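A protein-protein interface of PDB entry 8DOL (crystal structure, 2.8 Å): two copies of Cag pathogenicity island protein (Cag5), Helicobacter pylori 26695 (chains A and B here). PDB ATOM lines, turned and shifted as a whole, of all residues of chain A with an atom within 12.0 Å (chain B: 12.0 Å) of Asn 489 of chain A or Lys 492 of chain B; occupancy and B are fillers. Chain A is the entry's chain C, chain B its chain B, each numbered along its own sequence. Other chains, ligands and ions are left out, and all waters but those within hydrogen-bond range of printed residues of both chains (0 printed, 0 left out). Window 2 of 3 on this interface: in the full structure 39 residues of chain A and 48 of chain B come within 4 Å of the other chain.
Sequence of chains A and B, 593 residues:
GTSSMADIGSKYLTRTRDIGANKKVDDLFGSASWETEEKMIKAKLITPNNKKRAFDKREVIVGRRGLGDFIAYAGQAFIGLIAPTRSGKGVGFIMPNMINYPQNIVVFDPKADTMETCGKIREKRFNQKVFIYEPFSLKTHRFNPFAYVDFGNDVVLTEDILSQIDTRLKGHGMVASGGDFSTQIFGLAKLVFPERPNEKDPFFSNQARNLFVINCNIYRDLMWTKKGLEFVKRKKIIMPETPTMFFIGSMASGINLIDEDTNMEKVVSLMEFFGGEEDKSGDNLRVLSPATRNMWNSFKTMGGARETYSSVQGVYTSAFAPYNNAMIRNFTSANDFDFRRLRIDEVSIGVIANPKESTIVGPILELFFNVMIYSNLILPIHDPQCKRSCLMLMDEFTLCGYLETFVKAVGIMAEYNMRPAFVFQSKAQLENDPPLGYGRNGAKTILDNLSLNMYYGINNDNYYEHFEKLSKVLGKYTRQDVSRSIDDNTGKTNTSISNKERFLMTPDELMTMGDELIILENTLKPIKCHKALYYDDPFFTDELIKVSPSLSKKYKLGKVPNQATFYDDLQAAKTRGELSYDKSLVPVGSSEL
The backbone NH (N) of Asp 488 of chain A lies within hydrogen-bond range of the backbone carbonyl oxygen (O) of Thr 493 of chain B, at 3.0 Å.
O of Thr 495 of chain B is in hydrogen-bond range of N of Ile 486 of chain A, at 2.4 Å.
OD2 of Asp 488 of chain A is in hydrogen-bond range of OG1 of Thr 495 of chain B, at 2.9 Å.
OD2 of Asp 488 of chain A lies close to NH2 of Arg 484 of chain B, at 2.3 Å.
Ile 486 of chain A touches Asn 494 of chain B, but with the chains exchanged Asn 494 of chain A does not touch Ile 486 of chain B (14.0 Å).
Asp 487 of chain A touches Asn 494 of chain B, but with the chains exchanged Asn 494 of chain A does not touch Asp 487 of chain B (14.7 Å).
Asp 488 of chain A touches Thr 493 of chain B, but with the chains exchanged Thr 493 of chain A does not touch Asp 488 of chain B (19.3 Å).
Asn 489 of chain A touches Thr 493 of chain B, but with the chains exchanged Thr 493 of chain A does not touch Asn 489 of chain B (20.5 Å).
Of the 12 pairs that touch across the chains among the printed residues, none has its exchanged pair printed and touching as well.
Among the printed residues, merely in contact across the chains: Ser 485 of chain A with Thr 495 of chain B (3.1 Å), Ile 486 of chain A with Asn 494 of chain B (3.3 Å), Asn 489 of chain A with Lys 492 of chain B (3.5 Å), Asp 487 of chain A with Asn 494 of chain B (3.6 Å), Ser 485 of chain A with Ser 496 of chain B (3.6 Å), Asp 487 of chain A with Thr 493 of chain B (3.9 Å), Asn 489 of chain A with Thr 493 of chain B (3.97 Å) and Asp 488 of chain A with Asn 494 of chain B (3.98 Å).
Asn 489 of chain A touches two residues of chain B.
Lys 492 of chain B touches just one residue of chain A: Asn 489 (3.5 Å).
Asp 487 of chain A touches just these residues of chain B: Thr 493 (3.9 Å) and Asn 494 (3.6 Å).
Of chain B, only Arg 484 (2.3 Å), Thr 493 (3.0 Å), Asn 494 (3.98 Å) and Thr 495 (2.9 Å) come within 4 Å of Asp 488 of chain A.
No residue of chain B comes within 4 Å of Gly 491 of chain A.
No residue of chain A comes within 4 Å of Ser 485 of chain B.
No residue of chain A comes within 4 Å of Ile 486 of chain B.
No residue of chain A comes within 4 Å of Thr 490 of chain B.
No residue of chain A comes within 4 Å of Gly 491 of chain B.
Of the printed residues of chain A, Thr 495 of chain B touches Ser 485 (3.1 Å), Ile 486 (2.4 Å) and Asp 488 (2.9 Å).
Of the printed residues of chain B, Ser 485 of chain A touches Thr 495 (3.1 Å) and Ser 496 (3.6 Å).
Printed residues of chain A within 4 Å of Arg 484 of chain B: Asp 488.
Of the printed residues of chain A, Ser 496 of chain B touches Ser 485.
Asp 488 of chain B touches none of the printed residues of chain A.
The nearest residue of chain A that does not touch Lys 492 of chain B is Asp 487 of chain A (5.4 Å).
The backbone NH of Ser 483 of chain B lies within hydrogen-bond range of the backbone carbonyl oxygen of Ser 496 of chain B, 2.9 Å away.
NE of Arg 484 of chain B sits at hydrogen-bond distance from OG1 of Thr 495 of chain B (2.9 Å).
The backbone NH (N) of Asn 494 of chain B sits at hydrogen-bond distance from the backbone carbonyl oxygen (O) of Ser 485 of chain B.
OG1 of Thr 490 of chain B lies close to N of Lys 492 of chain B (3.2 Å).
The side-chain carboxylate of Asp 487 of chain A lies close to the backbone NH of Asn 489 of chain A, at 3.3 Å.
The backbone carbonyl oxygen (O) of Lys 492 of chain A is in hydrogen-bond range of the backbone NH (N) of Asp 487 of chain A (3.0 Å).
Of the 14 printed residues of chain B, 6 touch a printed residue of chain A.
Printed residues of chain A that touch a printed residue of chain B: Ser 485, Ile 486, Asp 487, Asp 488 and Asn 489.
Hydrophobic or aromatic side chains of chain A within 4 Å of the printed part of chain B: Ile 486.
Among the printed residues, Asp or Glu carboxylates within 4 Å of a Lys or Arg side-chain nitrogen of the other chain: Asp 488 of chain A with Arg 484 of chain B (2.3 Å).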
ATOM      1  N   SER A 485     -26.470 -28.234 -12.704  1.00  0.00           N
ATOM      2  CA  SER A 485     -25.605 -27.917 -11.576  1.00  0.00           C
ATOM      3  C   SER A 485     -26.121 -26.663 -10.891  1.00  0.00           C
ATOM      4  O   SER A 485     -26.444 -25.680 -11.559  1.00  0.00           O
ATOM      5  CB  SER A 485     -24.151 -27.729 -12.025  1.00  0.00           C
ATOM      6  OG  SER A 485     -23.913 -26.402 -12.456  1.00  0.00           O
ATOM      7  N   ILE A 486     -26.202 -26.697  -9.562  1.00  0.00           N
ATOM      8  CA  ILE A 486     -26.781 -25.612  -8.779  1.00  0.00           C
ATOM      9  C   ILE A 486     -25.686 -24.965  -7.943  1.00  0.00           C
ATOM     10  O   ILE A 486     -24.827 -25.657  -7.384  1.00  0.00           O
ATOM     11  CB  ILE A 486     -27.930 -26.095  -7.868  1.00  0.00           C
ATOM     12  CG1 ILE A 486     -28.667 -27.310  -8.453  1.00  0.00           C
ATOM     13  CG2 ILE A 486     -28.913 -24.964  -7.619  1.00  0.00           C
ATOM     14  CD1 ILE A 486     -29.324 -27.087  -9.809  1.00  0.00           C
ATOM     15  N   ASP A 487     -25.721 -23.638  -7.852  1.00  0.00           N
ATOM     16  CA  ASP A 487     -24.869 -22.899  -6.923  1.00  0.00           C
ATOM     17  C   ASP A 487     -25.644 -22.765  -5.619  1.00  0.00           C
ATOM     18  O   ASP A 487     -26.550 -21.936  -5.502  1.00  0.00           O
ATOM     19  CB  ASP A 487     -24.477 -21.543  -7.499  1.00  0.00           C
ATOM     20  CG  ASP A 487     -23.523 -20.781  -6.599  1.00  0.00           C
ATOM     21  OD1 ASP A 487     -23.924 -20.418  -5.471  1.00  0.00           O
ATOM     22  OD2 ASP A 487     -22.367 -20.554  -7.015  1.00  0.00           O
ATOM     23  N   ASP A 488     -25.283 -23.587  -4.630  1.00  0.00           N
ATOM     24  CA  ASP A 488     -26.096 -23.713  -3.424  1.00  0.00           C
ATOM     25  C   ASP A 488     -26.169 -22.413  -2.636  1.00  0.00           C
ATOM     26  O   ASP A 488     -27.183 -22.143  -1.984  1.00  0.00           O
ATOM     27  CB  ASP A 488     -25.549 -24.829  -2.537  1.00  0.00           C
ATOM     28  CG  ASP A 488     -25.722 -26.196  -3.154  1.00  0.00           C
ATOM     29  OD1 ASP A 488     -26.725 -26.405  -3.868  1.00  0.00           O
ATOM     30  OD2 ASP A 488     -24.854 -27.063  -2.923  1.00  0.00           O
ATOM     31  N   ASN A 489     -25.111 -21.602  -2.672  1.00  0.00           N
ATOM     32  CA  ASN A 489     -25.112 -20.372  -1.888  1.00  0.00           C
ATOM     33  C   ASN A 489     -26.118 -19.366  -2.435  1.00  0.00           C
ATOM     34  O   ASN A 489     -26.779 -18.660  -1.664  1.00  0.00           O
ATOM     35  CB  ASN A 489     -23.710 -19.767  -1.852  1.00  0.00           C
ATOM     36  CG  ASN A 489     -23.353 -19.213  -0.486  1.00  0.00           C
ATOM     37  OD1 ASN A 489     -23.202 -19.962   0.479  1.00  0.00           O
ATOM     38  ND2 ASN A 489     -23.220 -17.894  -0.398  1.00  0.00           N
ATOM     39  N   THR A 490     -26.256 -19.291  -3.757  1.00  0.00           N
ATOM     40  CA  THR A 490     -27.167 -18.349  -4.396  1.00  0.00           C
ATOM     41  C   THR A 490     -28.447 -19.014  -4.891  1.00  0.00           C
ATOM     42  O   THR A 490     -29.547 -18.571  -4.552  1.00  0.00           O
ATOM     43  CB  THR A 490     -26.466 -17.650  -5.566  1.00  0.00           C
ATOM     44  OG1 THR A 490     -26.642 -18.423  -6.761  1.00  0.00           O
ATOM     45  CG2 THR A 490     -24.981 -17.490  -5.280  1.00  0.00           C
ATOM     46  N   GLY A 491     -28.323 -20.071  -5.686  1.00  0.00           N
ATOM     47  CA  GLY A 491     -29.464 -20.728  -6.296  1.00  0.00           C
ATOM     48  C   GLY A 491     -29.477 -20.679  -7.808  1.00  0.00           C
ATOM     49  O   GLY A 491     -30.309 -21.362  -8.426  1.00  0.00           O
ATOM     50  N   LYS A 492     -28.599 -19.898  -8.435  1.00  0.00           N
ATOM     51  CA  LYS A 492     -28.516 -19.883  -9.888  1.00  0.00           C
ATOM     52  C   LYS A 492     -28.066 -21.247 -10.400  1.00  0.00           C
ATOM     53  O   LYS A 492     -27.258 -21.933  -9.767  1.00  0.00           O
ATOM     54  CB  LYS A 492     -27.551 -18.792 -10.354  1.00  0.00           C
ATOM     55  CG  LYS A 492     -27.705 -17.467  -9.617  1.00  0.00           C
ATOM     56  CD  LYS A 492     -28.843 -16.634 -10.192  1.00  0.00           C
ATOM     57  CE  LYS A 492     -28.316 -15.440 -10.974  1.00  0.00           C
ATOM     58  NZ  LYS A 492     -29.415 -14.573 -11.486  1.00  0.00           N
ATOM     59  N   THR A 493     -28.599 -21.643 -11.550  1.00  0.00           N
ATOM     60  CA  THR A 493     -28.391 -22.981 -12.077  1.00  0.00           C
ATOM     61  C   THR A 493     -27.656 -22.933 -13.411  1.00  0.00           C
ATOM     62  O   THR A 493     -27.518 -21.884 -14.045  1.00  0.00           O
ATOM     63  CB  THR A 493     -29.726 -23.723 -12.235  1.00  0.00           C
ATOM     64  OG1 THR A 493     -30.369 -23.300 -13.442  1.00  0.00           O
ATOM     65  CG2 THR A 493     -30.637 -23.442 -11.051  1.00  0.00           C
ATOM     66  N   ASN A 494     -27.183 -24.107 -13.821  1.00  0.00           N
ATOM     67  CA  ASN A 494     -26.452 -24.305 -15.063  1.00  0.00           C
ATOM     68  C   ASN A 494     -26.967 -25.576 -15.713  1.00  0.00           C
ATOM     69  O   ASN A 494     -27.077 -26.610 -15.048  1.00  0.00           O
ATOM     70  CB  ASN A 494     -24.945 -24.426 -14.813  1.00  0.00           C
ATOM     71  CG  ASN A 494     -24.213 -23.116 -14.998  1.00  0.00           C
ATOM     72  OD1 ASN A 494     -23.006 -23.099 -15.235  1.00  0.00           O
ATOM     73  ND2 ASN A 494     -24.937 -22.010 -14.887  1.00  0.00           N
ATOM     74  N   SER B 483     -22.921 -34.847  -7.588  1.00  0.00           N
ATOM     75  CA  SER B 483     -21.561 -34.475  -7.230  1.00  0.00           C
ATOM     76  C   SER B 483     -21.576 -33.106  -6.566  1.00  0.00           C
ATOM     77  O   SER B 483     -22.492 -32.303  -6.768  1.00  0.00           O
ATOM     78  CB  SER B 483     -20.637 -34.460  -8.455  1.00  0.00           C
ATOM     79  OG  SER B 483     -20.986 -35.482  -9.373  1.00  0.00           O
ATOM     80  N   ARG B 484     -20.551 -32.842  -5.761  1.00  0.00           N
ATOM     81  CA  ARG B 484     -20.456 -31.599  -5.011  1.00  0.00           C
ATOM     82  C   ARG B 484     -19.065 -31.004  -5.165  1.00  0.00           C
ATOM     83  O   ARG B 484     -18.071 -31.725  -5.283  1.00  0.00           O
ATOM     84  CB  ARG B 484     -20.766 -31.815  -3.520  1.00  0.00           C
ATOM     85  CG  ARG B 484     -21.902 -32.793  -3.253  1.00  0.00           C
ATOM     86  CD  ARG B 484     -22.924 -32.212  -2.293  1.00  0.00           C
ATOM     87  NE  ARG B 484     -23.075 -30.772  -2.463  1.00  0.00           N
ATOM     88  CZ  ARG B 484     -23.500 -29.949  -1.514  1.00  0.00           C
ATOM     89  NH1 ARG B 484     -23.833 -30.394  -0.313  1.00  0.00           N
ATOM     90  NH2 ARG B 484     -23.590 -28.649  -1.775  1.00  0.00           N
ATOM     91  N   SER B 485     -19.011 -29.676  -5.166  1.00  0.00           N
ATOM     92  CA  SER B 485     -17.763 -28.930  -5.202  1.00  0.00           C
ATOM     93  C   SER B 485     -17.799 -27.855  -4.127  1.00  0.00           C
ATOM     94  O   SER B 485     -18.867 -27.365  -3.757  1.00  0.00           O
ATOM     95  CB  SER B 485     -17.521 -28.289  -6.575  1.00  0.00           C
ATOM     96  OG  SER B 485     -17.483 -29.272  -7.595  1.00  0.00           O
ATOM     97  N   ILE B 486     -16.623 -27.485  -3.630  1.00  0.00           N
ATOM     98  CA  ILE B 486     -16.510 -26.477  -2.582  1.00  0.00           C
ATOM     99  C   ILE B 486     -15.261 -25.644  -2.833  1.00  0.00           C
ATOM    100  O   ILE B 486     -14.186 -26.191  -3.102  1.00  0.00           O
ATOM    101  CB  ILE B 486     -16.469 -27.110  -1.176  1.00  0.00           C
ATOM    102  CG1 ILE B 486     -16.057 -26.074  -0.127  1.00  0.00           C
ATOM    103  CG2 ILE B 486     -15.530 -28.307  -1.147  1.00  0.00           C
ATOM    104  CD1 ILE B 486     -16.227 -26.550   1.295  1.00  0.00           C
ATOM    105  N   ASP B 487     -15.409 -24.324  -2.761  1.00  0.00           N
ATOM    106  CA  ASP B 487     -14.263 -23.425  -2.762  1.00  0.00           C
ATOM    107  C   ASP B 487     -13.629 -23.447  -1.378  1.00  0.00           C
ATOM    108  O   ASP B 487     -14.254 -23.030  -0.397  1.00  0.00           O
ATOM    109  CB  ASP B 487     -14.695 -22.011  -3.143  1.00  0.00           C
ATOM    110  CG  ASP B 487     -13.520 -21.067  -3.316  1.00  0.00           C
ATOM    111  OD1 ASP B 487     -12.557 -21.153  -2.524  1.00  0.00           O
ATOM    112  OD2 ASP B 487     -13.562 -20.234  -4.247  1.00  0.00           O
ATOM    113  N   ASP B 488     -12.393 -23.939  -1.296  1.00  0.00           N
ATOM    114  CA  ASP B 488     -11.729 -24.104  -0.007  1.00  0.00           C
ATOM    115  C   ASP B 488     -11.450 -22.784   0.698  1.00  0.00           C
ATOM    116  O   ASP B 488     -11.131 -22.799   1.891  1.00  0.00           O
ATOM    117  CB  ASP B 488     -10.424 -24.879  -0.191  1.00  0.00           C
ATOM    118  CG  ASP B 488     -10.620 -26.169  -0.957  1.00  0.00           C
ATOM    119  OD1 ASP B 488     -11.488 -26.971  -0.554  1.00  0.00           O
ATOM    120  OD2 ASP B 488      -9.908 -26.384  -1.960  1.00  0.00           O
ATOM    121  N   ASN B 489     -11.558 -21.654   0.000  1.00  0.00           N
ATOM    122  CA  ASN B 489     -11.357 -20.346   0.615  1.00  0.00           C
ATOM    123  C   ASN B 489     -12.665 -19.786   1.171  1.00  0.00           C
ATOM    124  O   ASN B 489     -12.792 -19.568   2.380  1.00  0.00           O
ATOM    125  CB  ASN B 489     -10.743 -19.376  -0.401  1.00  0.00           C
ATOM    126  CG  ASN B 489      -9.344 -18.934  -0.014  1.00  0.00           C
ATOM    127  OD1 ASN B 489      -9.113 -18.474   1.105  1.00  0.00           O
ATOM    128  ND2 ASN B 489      -8.402 -19.074  -0.940  1.00  0.00           N
ATOM    129  N   THR B 490     -13.648 -19.561   0.298  1.00  0.00           N
ATOM    130  CA  THR B 490     -14.911 -18.968   0.725  1.00  0.00           C
ATOM    131  C   THR B 490     -15.775 -19.972   1.479  1.00  0.00           C
ATOM    132  O   THR B 490     -16.336 -19.653   2.532  1.00  0.00           O
ATOM    133  CB  THR B 490     -15.668 -18.415  -0.484  1.00  0.00           C
ATOM    134  OG1 THR B 490     -16.215 -19.499  -1.244  1.00  0.00           O
ATOM    135  CG2 THR B 490     -14.734 -17.606  -1.373  1.00  0.00           C
ATOM    136  N   GLY B 491     -15.897 -21.188   0.956  1.00  0.00           N
ATOM    137  CA  GLY B 491     -16.733 -22.206   1.550  1.00  0.00           C
ATOM    138  C   GLY B 491     -18.031 -22.465   0.819  1.00  0.00           C
ATOM    139  O   GLY B 491     -18.764 -23.385   1.202  1.00  0.00           O
ATOM    140  N   LYS B 492     -18.341 -21.682  -0.213  1.00  0.00           N
ATOM    141  CA  LYS B 492     -19.557 -21.900  -0.980  1.00  0.00           C
ATOM    142  C   LYS B 492     -19.497 -23.242  -1.698  1.00  0.00           C
ATOM    143  O   LYS B 492     -18.427 -23.721  -2.083  1.00  0.00           O
ATOM    144  CB  LYS B 492     -19.763 -20.771  -1.989  1.00  0.00           C
ATOM    145  CG  LYS B 492     -19.373 -19.397  -1.473  1.00  0.00           C
ATOM    146  CD  LYS B 492     -19.066 -18.441  -2.616  1.00  0.00           C
ATOM    147  CE  LYS B 492     -20.134 -17.365  -2.744  1.00  0.00           C
ATOM    148  NZ  LYS B 492     -20.203 -16.494  -1.535  1.00  0.00           N
ATOM    149  N   THR B 493     -20.665 -23.851  -1.877  1.00  0.00           N
ATOM    150  CA  THR B 493     -20.771 -25.182  -2.450  1.00  0.00           C
ATOM    151  C   THR B 493     -21.593 -25.149  -3.731  1.00  0.00           C
ATOM    152  O   THR B 493     -22.471 -24.300  -3.909  1.00  0.00           O
ATOM    153  CB  THR B 493     -21.404 -26.167  -1.459  1.00  0.00           C
ATOM    154  OG1 THR B 493     -22.751 -25.768  -1.179  1.00  0.00           O
ATOM    155  CG2 THR B 493     -20.610 -26.196  -0.163  1.00  0.00           C
ATOM    156  N   ASN B 494     -21.289 -26.089  -4.622  1.00  0.00           N
ATOM    157  CA  ASN B 494     -21.985 -26.254  -5.891  1.00  0.00           C
ATOM    158  C   ASN B 494     -22.423 -27.705  -6.008  1.00  0.00           C
ATOM    159  O   ASN B 494     -21.628 -28.616  -5.760  1.00  0.00           O
ATOM    160  CB  ASN B 494     -21.090 -25.876  -7.077  1.00  0.00           C
ATOM    161  CG  ASN B 494     -20.714 -24.404  -7.081  1.00  0.00           C
ATOM    162  OD1 ASN B 494     -20.088 -23.909  -6.140  1.00  0.00           O
ATOM    163  ND2 ASN B 494     -21.089 -23.699  -8.140  1.00  0.00           N
ATOM    164  N   THR B 495     -23.684 -27.918  -6.375  1.00  0.00           N
ATOM    165  CA  THR B 495     -24.257 -29.252  -6.492  1.00  0.00           C
ATOM    166  C   THR B 495     -24.608 -29.519  -7.949  1.00  0.00           C
ATOM    167  O   THR B 495     -25.341 -28.738  -8.565  1.00  0.00           O
ATOM    168  CB  THR B 495     -25.502 -29.392  -5.607  1.00  0.00           C
ATOM    169  OG1 THR B 495     -25.103 -29.653  -4.257  1.00  0.00           O
ATOM    170  CG2 THR B 495     -26.383 -30.531  -6.094  1.00  0.00           C
ATOM    171  N   SER B 496     -24.091 -30.619  -8.495  1.00  0.00           N
ATOM    172  CA  SER B 496     -24.325 -31.001  -9.880  1.00  0.00           C
ATOM    173  C   SER B 496     -25.047 -32.339  -9.934  1.00  0.00           C
ATOM    174  O   SER B 496     -24.752 -33.247  -9.151  1.00  0.00           O
ATOM    175  CB  SER B 496     -23.006 -31.086 -10.659  1.00  0.00           C
ATOM    176  OG  SER B 496     -22.092 -30.097 -10.221  1.00  0.00           O
